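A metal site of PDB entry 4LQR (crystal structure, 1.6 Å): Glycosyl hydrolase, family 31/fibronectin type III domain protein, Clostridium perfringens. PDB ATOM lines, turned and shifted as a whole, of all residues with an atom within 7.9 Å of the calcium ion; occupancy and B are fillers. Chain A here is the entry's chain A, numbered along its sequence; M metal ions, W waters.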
ATOM      1  N   ASP A  22     -15.372  11.797  21.257  1.00  0.00           N
ATOM      2  CA  ASP A  22     -16.751  11.417  21.475  1.00  0.00           C
ATOM      3  C   ASP A  22     -17.477  11.271  20.120  1.00  0.00           C
ATOM      4  O   ASP A  22     -17.273  12.067  19.188  1.00  0.00           O
ATOM      5  CB  ASP A  22     -17.505  12.493  22.260  1.00  0.00           C
ATOM      6  CG  ASP A  22     -17.095  12.545  23.740  1.00  0.00           C
ATOM      7  OD1 ASP A  22     -16.932  11.536  24.367  1.00  0.00           O
ATOM      8  OD2 ASP A  22     -16.950  13.565  24.216  1.00  0.00           O
ATOM      9  N   SER A  23     -18.393  10.283  20.009  1.00  0.00           N
ATOM     10  CA  SER A  23     -18.993  10.079  18.675  1.00  0.00           C
ATOM     11  C   SER A  23     -19.911  11.212  18.223  1.00  0.00           C
ATOM     12  O   SER A  23     -20.118  11.358  17.014  1.00  0.00           O
ATOM     13  CB  SER A  23     -19.722   8.731  18.569  1.00  0.00           C
ATOM     14  OG  SER A  23     -18.809   7.664  18.704  1.00  0.00           O
ATOM     15  N   SER A  24     -20.431  12.038  19.155  1.00  0.00           N
ATOM     16  CA  SER A  24     -21.247  13.193  18.759  1.00  0.00           C
ATOM     17  C   SER A  24     -20.435  14.246  17.959  1.00  0.00           C
ATOM     18  O   SER A  24     -21.060  15.093  17.335  1.00  0.00           O
ATOM     19  CB  SER A  24     -21.835  13.921  20.016  1.00  0.00           C
ATOM     20  OG  SER A  24     -20.806  14.371  20.858  1.00  0.00           O
ATOM     21  N   LYS A  25     -19.110  14.138  18.054  1.00  0.00           N
ATOM     22  CA  LYS A  25     -18.210  14.994  17.259  1.00  0.00           C
ATOM     23  C   LYS A  25     -18.015  14.527  15.841  1.00  0.00           C
ATOM     24  O   LYS A  25     -17.347  15.221  15.051  1.00  0.00           O
ATOM     25  CB  LYS A  25     -16.869  15.157  17.930  1.00  0.00           C
ATOM     26  CG  LYS A  25     -17.131  15.962  19.273  1.00  0.00           C
ATOM     27  CD  LYS A  25     -16.002  15.803  20.117  1.00  0.00           C
ATOM     28  CE  LYS A  25     -16.295  16.447  21.494  1.00  0.00           C
ATOM     29  NZ  LYS A  25     -16.753  17.892  21.604  1.00  0.00           N
ATOM     30  N   LEU A  26     -18.660  13.382  15.503  1.00  0.00           N
ATOM     31  CA  LEU A  26     -18.455  12.772  14.155  1.00  0.00           C
ATOM     32  C   LEU A  26     -19.766  12.757  13.450  1.00  0.00           C
ATOM     33  O   LEU A  26     -20.749  12.157  13.943  1.00  0.00           O
ATOM     34  CB  LEU A  26     -17.997  11.337  14.342  1.00  0.00           C
ATOM     35  CG  LEU A  26     -16.520  11.097  14.656  1.00  0.00           C
ATOM     36  CD1 LEU A  26     -16.112  11.888  15.916  1.00  0.00           C
ATOM     37  CD2 LEU A  26     -16.329   9.581  14.826  1.00  0.00           C
ATOM     38  N   GLU A  27     -19.811  13.402  12.275  1.00  0.00           N
ATOM     39  CA  GLU A  27     -21.049  13.440  11.458  1.00  0.00           C
ATOM     40  C   GLU A  27     -20.752  12.710  10.165  1.00  0.00           C
ATOM     41  O   GLU A  27     -19.873  13.092   9.401  1.00  0.00           O
ATOM     42  CB  GLU A  27     -21.496  14.881  11.179  1.00  0.00           C
ATOM     43  CG  GLU A  27     -22.761  14.957  10.369  1.00  0.00           C
ATOM     44  CD  GLU A  27     -23.080  16.356   9.900  1.00  0.00           C
ATOM     45  OE1 GLU A  27     -22.327  17.319  10.159  1.00  0.00           O
ATOM     46  OE2 GLU A  27     -24.064  16.456   9.105  1.00  0.00           O
ATOM     47  N   ALA A  28     -21.530  11.672   9.856  1.00  0.00           N
ATOM     48  CA  ALA A  28     -21.397  11.031   8.528  1.00  0.00           C
ATOM     49  C   ALA A  28     -22.150  11.883   7.501  1.00  0.00           C
ATOM     50  O   ALA A  28     -23.396  11.991   7.554  1.00  0.00           O
ATOM     51  CB  ALA A  28     -21.979   9.623   8.541  1.00  0.00           C
ATOM     52  N   LYS A  40     -25.702   5.760   7.156  1.00  0.00           N
ATOM     53  CA  LYS A  40     -24.300   6.220   7.349  1.00  0.00           C
ATOM     54  C   LYS A  40     -24.050   6.750   8.777  1.00  0.00           C
ATOM     55  O   LYS A  40     -22.975   6.498   9.323  1.00  0.00           O
ATOM     56  CB  LYS A  40     -23.913   7.190   6.207  1.00  0.00           C
ATOM     57  CG  LYS A  40     -24.713   8.454   6.223  1.00  0.00           C
ATOM     58  CD  LYS A  40     -24.371   9.350   5.044  1.00  0.00           C
ATOM     59  CE  LYS A  40     -25.096  10.694   5.018  1.00  0.00           C
ATOM     60  NZ  LYS A  40     -26.531  10.479   4.587  1.00  0.00           N
ATOM     61  N   GLU A  41     -25.019   7.438   9.352  1.00  0.00           N
ATOM     62  CA  GLU A  41     -24.824   8.036  10.688  1.00  0.00           C
ATOM     63  C   GLU A  41     -24.538   6.924  11.704  1.00  0.00           C
ATOM     64  O   GLU A  41     -23.894   7.171  12.713  1.00  0.00           O
ATOM     65  CB  GLU A  41     -26.038   8.805  11.129  1.00  0.00           C
ATOM     66  CG  GLU A  41     -26.383  10.097  10.305  1.00  0.00           C
ATOM     67  CD  GLU A  41     -27.065   9.863   8.978  1.00  0.00           C
ATOM     68  OE1 GLU A  41     -27.410   8.698   8.627  1.00  0.00           O
ATOM     69  OE2 GLU A  41     -27.179  10.863   8.173  1.00  0.00           O
ATOM     70  N   ASN A  42     -24.997   5.702  11.444  1.00  0.00           N
ATOM     71  CA  ASN A  42     -24.829   4.633  12.410  1.00  0.00           C
ATOM     72  C   ASN A  42     -23.376   4.164  12.447  1.00  0.00           C
ATOM     73  O   ASN A  42     -23.008   3.401  13.410  1.00  0.00           O
ATOM     74  CB  ASN A  42     -25.648   3.414  12.057  1.00  0.00           C
ATOM     75  CG  ASN A  42     -27.148   3.637  12.237  1.00  0.00           C
ATOM     76  OD1 ASN A  42     -27.591   4.697  12.627  1.00  0.00           O
ATOM     77  ND2 ASN A  42     -27.954   2.616  11.872  1.00  0.00           N
ATOM     78  N   ALA A  43     -22.495   4.569  11.478  1.00  0.00           N
ATOM     79  CA  ALA A  43     -21.109   4.160  11.585  1.00  0.00           C
ATOM     80  C   ALA A  43     -20.390   4.939  12.641  1.00  0.00           C
ATOM     81  O   ALA A  43     -19.293   4.574  13.002  1.00  0.00           O
ATOM     82  CB  ALA A  43     -20.360   4.365  10.246  1.00  0.00           C
ATOM     83  N   VAL A  44     -20.930   6.061  13.074  1.00  0.00           N
ATOM     84  CA  VAL A  44     -20.222   6.978  14.011  1.00  0.00           C
ATOM     85  C   VAL A  44     -21.182   7.533  15.066  1.00  0.00           C
ATOM     86  O   VAL A  44     -21.049   8.675  15.494  1.00  0.00           O
ATOM     87  CB  VAL A  44     -19.514   8.136  13.253  1.00  0.00           C
ATOM     88  CG1 VAL A  44     -18.354   7.601  12.432  1.00  0.00           C
ATOM     89  CG2 VAL A  44     -20.486   8.867  12.288  1.00  0.00           C
ATOM     90  N   ASP A  45     -22.072   6.651  15.550  1.00  0.00           N
ATOM     91  CA  ASP A  45     -23.049   7.080  16.590  1.00  0.00           C
ATOM     92  C   ASP A  45     -22.658   6.532  17.958  1.00  0.00           C
ATOM     93  O   ASP A  45     -23.457   6.780  18.912  1.00  0.00           O
ATOM     94  CB  ASP A  45     -24.467   6.679  16.242  1.00  0.00           C
ATOM     95  CG  ASP A  45     -24.647   5.132  16.142  1.00  0.00           C
ATOM     96  OD1 ASP A  45     -23.667   4.338  16.273  1.00  0.00           O
ATOM     97  OD2 ASP A  45     -25.804   4.742  15.894  1.00  0.00           O
ATOM     98  N   GLY A  46     -21.471   5.986  18.113  1.00  0.00           N
ATOM     99  CA  GLY A  46     -21.027   5.484  19.418  1.00  0.00           C
ATOM    100  C   GLY A  46     -21.787   4.289  19.893  1.00  0.00           C
ATOM    101  O   GLY A  46     -21.636   3.885  21.049  1.00  0.00           O
ATOM    102  N   ILE A  68     -16.755  11.142   6.933  1.00  0.00           N
ATOM    103  CA  ILE A  68     -17.076  11.661   8.252  1.00  0.00           C
ATOM    104  C   ILE A  68     -16.503  13.096   8.423  1.00  0.00           C
ATOM    105  O   ILE A  68     -15.323  13.348   8.104  1.00  0.00           O
ATOM    106  CB  ILE A  68     -16.365  10.783   9.322  1.00  0.00           C
ATOM    107  CG1 ILE A  68     -16.682   9.274   9.123  1.00  0.00           C
ATOM    108  CG2 ILE A  68     -16.689  11.251  10.760  1.00  0.00           C
ATOM    109  CD1 ILE A  68     -18.204   8.984   9.051  1.00  0.00           C
ATOM    110  N   LYS A  69     -17.357  14.011   8.881  1.00  0.00           N
ATOM    111  CA  LYS A  69     -16.947  15.399   9.234  1.00  0.00           C
ATOM    112  C   LYS A  69     -16.765  15.494  10.728  1.00  0.00           C
ATOM    113  O   LYS A  69     -17.674  15.106  11.471  1.00  0.00           O
ATOM    114  CB  LYS A  69     -18.048  16.338   8.815  1.00  0.00           C
ATOM    115  CG  LYS A  69     -17.673  17.813   9.197  1.00  0.00           C
ATOM    116  CD  LYS A  69     -18.815  18.727   8.805  1.00  0.00           C
ATOM    117  CE  LYS A  69     -18.395  20.127   9.258  1.00  0.00           C
ATOM    118  NZ  LYS A  69     -19.449  21.162   8.868  1.00  0.00           N
ATOM    119  N   GLU A 161     -18.793   0.727  14.023  1.00  0.00           N
ATOM    120  CA  GLU A 161     -18.262   1.992  14.517  1.00  0.00           C
ATOM    121  C   GLU A 161     -16.958   2.290  13.838  1.00  0.00           C
ATOM    122  O   GLU A 161     -16.164   1.384  13.543  1.00  0.00           O
ATOM    123  CB  GLU A 161     -17.964   1.866  16.051  1.00  0.00           C
ATOM    124  CG  GLU A 161     -19.257   2.056  16.883  1.00  0.00           C
ATOM    125  CD  GLU A 161     -19.950   3.421  16.653  1.00  0.00           C
ATOM    126  OE1 GLU A 161     -19.310   4.489  16.898  1.00  0.00           O
ATOM    127  OE2 GLU A 161     -21.105   3.513  16.239  1.00  0.00           O
ATOM    128  N   LEU A 162     -16.693   3.592  13.724  1.00  0.00           N
ATOM    129  CA  LEU A 162     -15.375   4.126  13.359  1.00  0.00           C
ATOM    130  C   LEU A 162     -14.998   5.040  14.514  1.00  0.00           C
ATOM    131  O   LEU A 162     -15.664   6.059  14.747  1.00  0.00           O
ATOM    132  CB  LEU A 162     -15.391   4.891  12.022  1.00  0.00           C
ATOM    133  CG  LEU A 162     -15.879   4.119  10.818  1.00  0.00           C
ATOM    134  CD1 LEU A 162     -15.913   5.081   9.653  1.00  0.00           C
ATOM    135  CD2 LEU A 162     -14.941   2.948  10.521  1.00  0.00           C
HETATM  136 CA    CA M   1     -21.870  10.847  15.532  1.00  0.00          CA
HETATM  137  O   HOH W   1     -23.350  12.770  15.615  1.00  0.00           O
HETATM  138  O   HOH W   2     -23.080  10.368  17.589  1.00  0.00           O
HETATM  139  O   HOH W   3     -23.643   9.707  14.066  1.00  0.00           O
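The side-chain hydroxyl of Ser 23 lies close to the backbone NH of Gly 46 (3.2 Å).
Within 4 Å of the calcium ion: Ser 23, Leu 26 and Val 44.
O of Val 44 is bound to the calcium ion, at 2.3 Å.
The backbone carbonyl oxygen (O) of Leu 26 binds the calcium ion (2.3 Å).
The backbone carbonyl oxygen (O) of Ser 23 is bound to the calcium ion, 2.4 Å away.
Water W1 binds the calcium ion, 2.4 Å away.
The calcium ion is bound by water W2 (2.4 Å).
Water W3 binds the calcium ion (2.6 Å).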
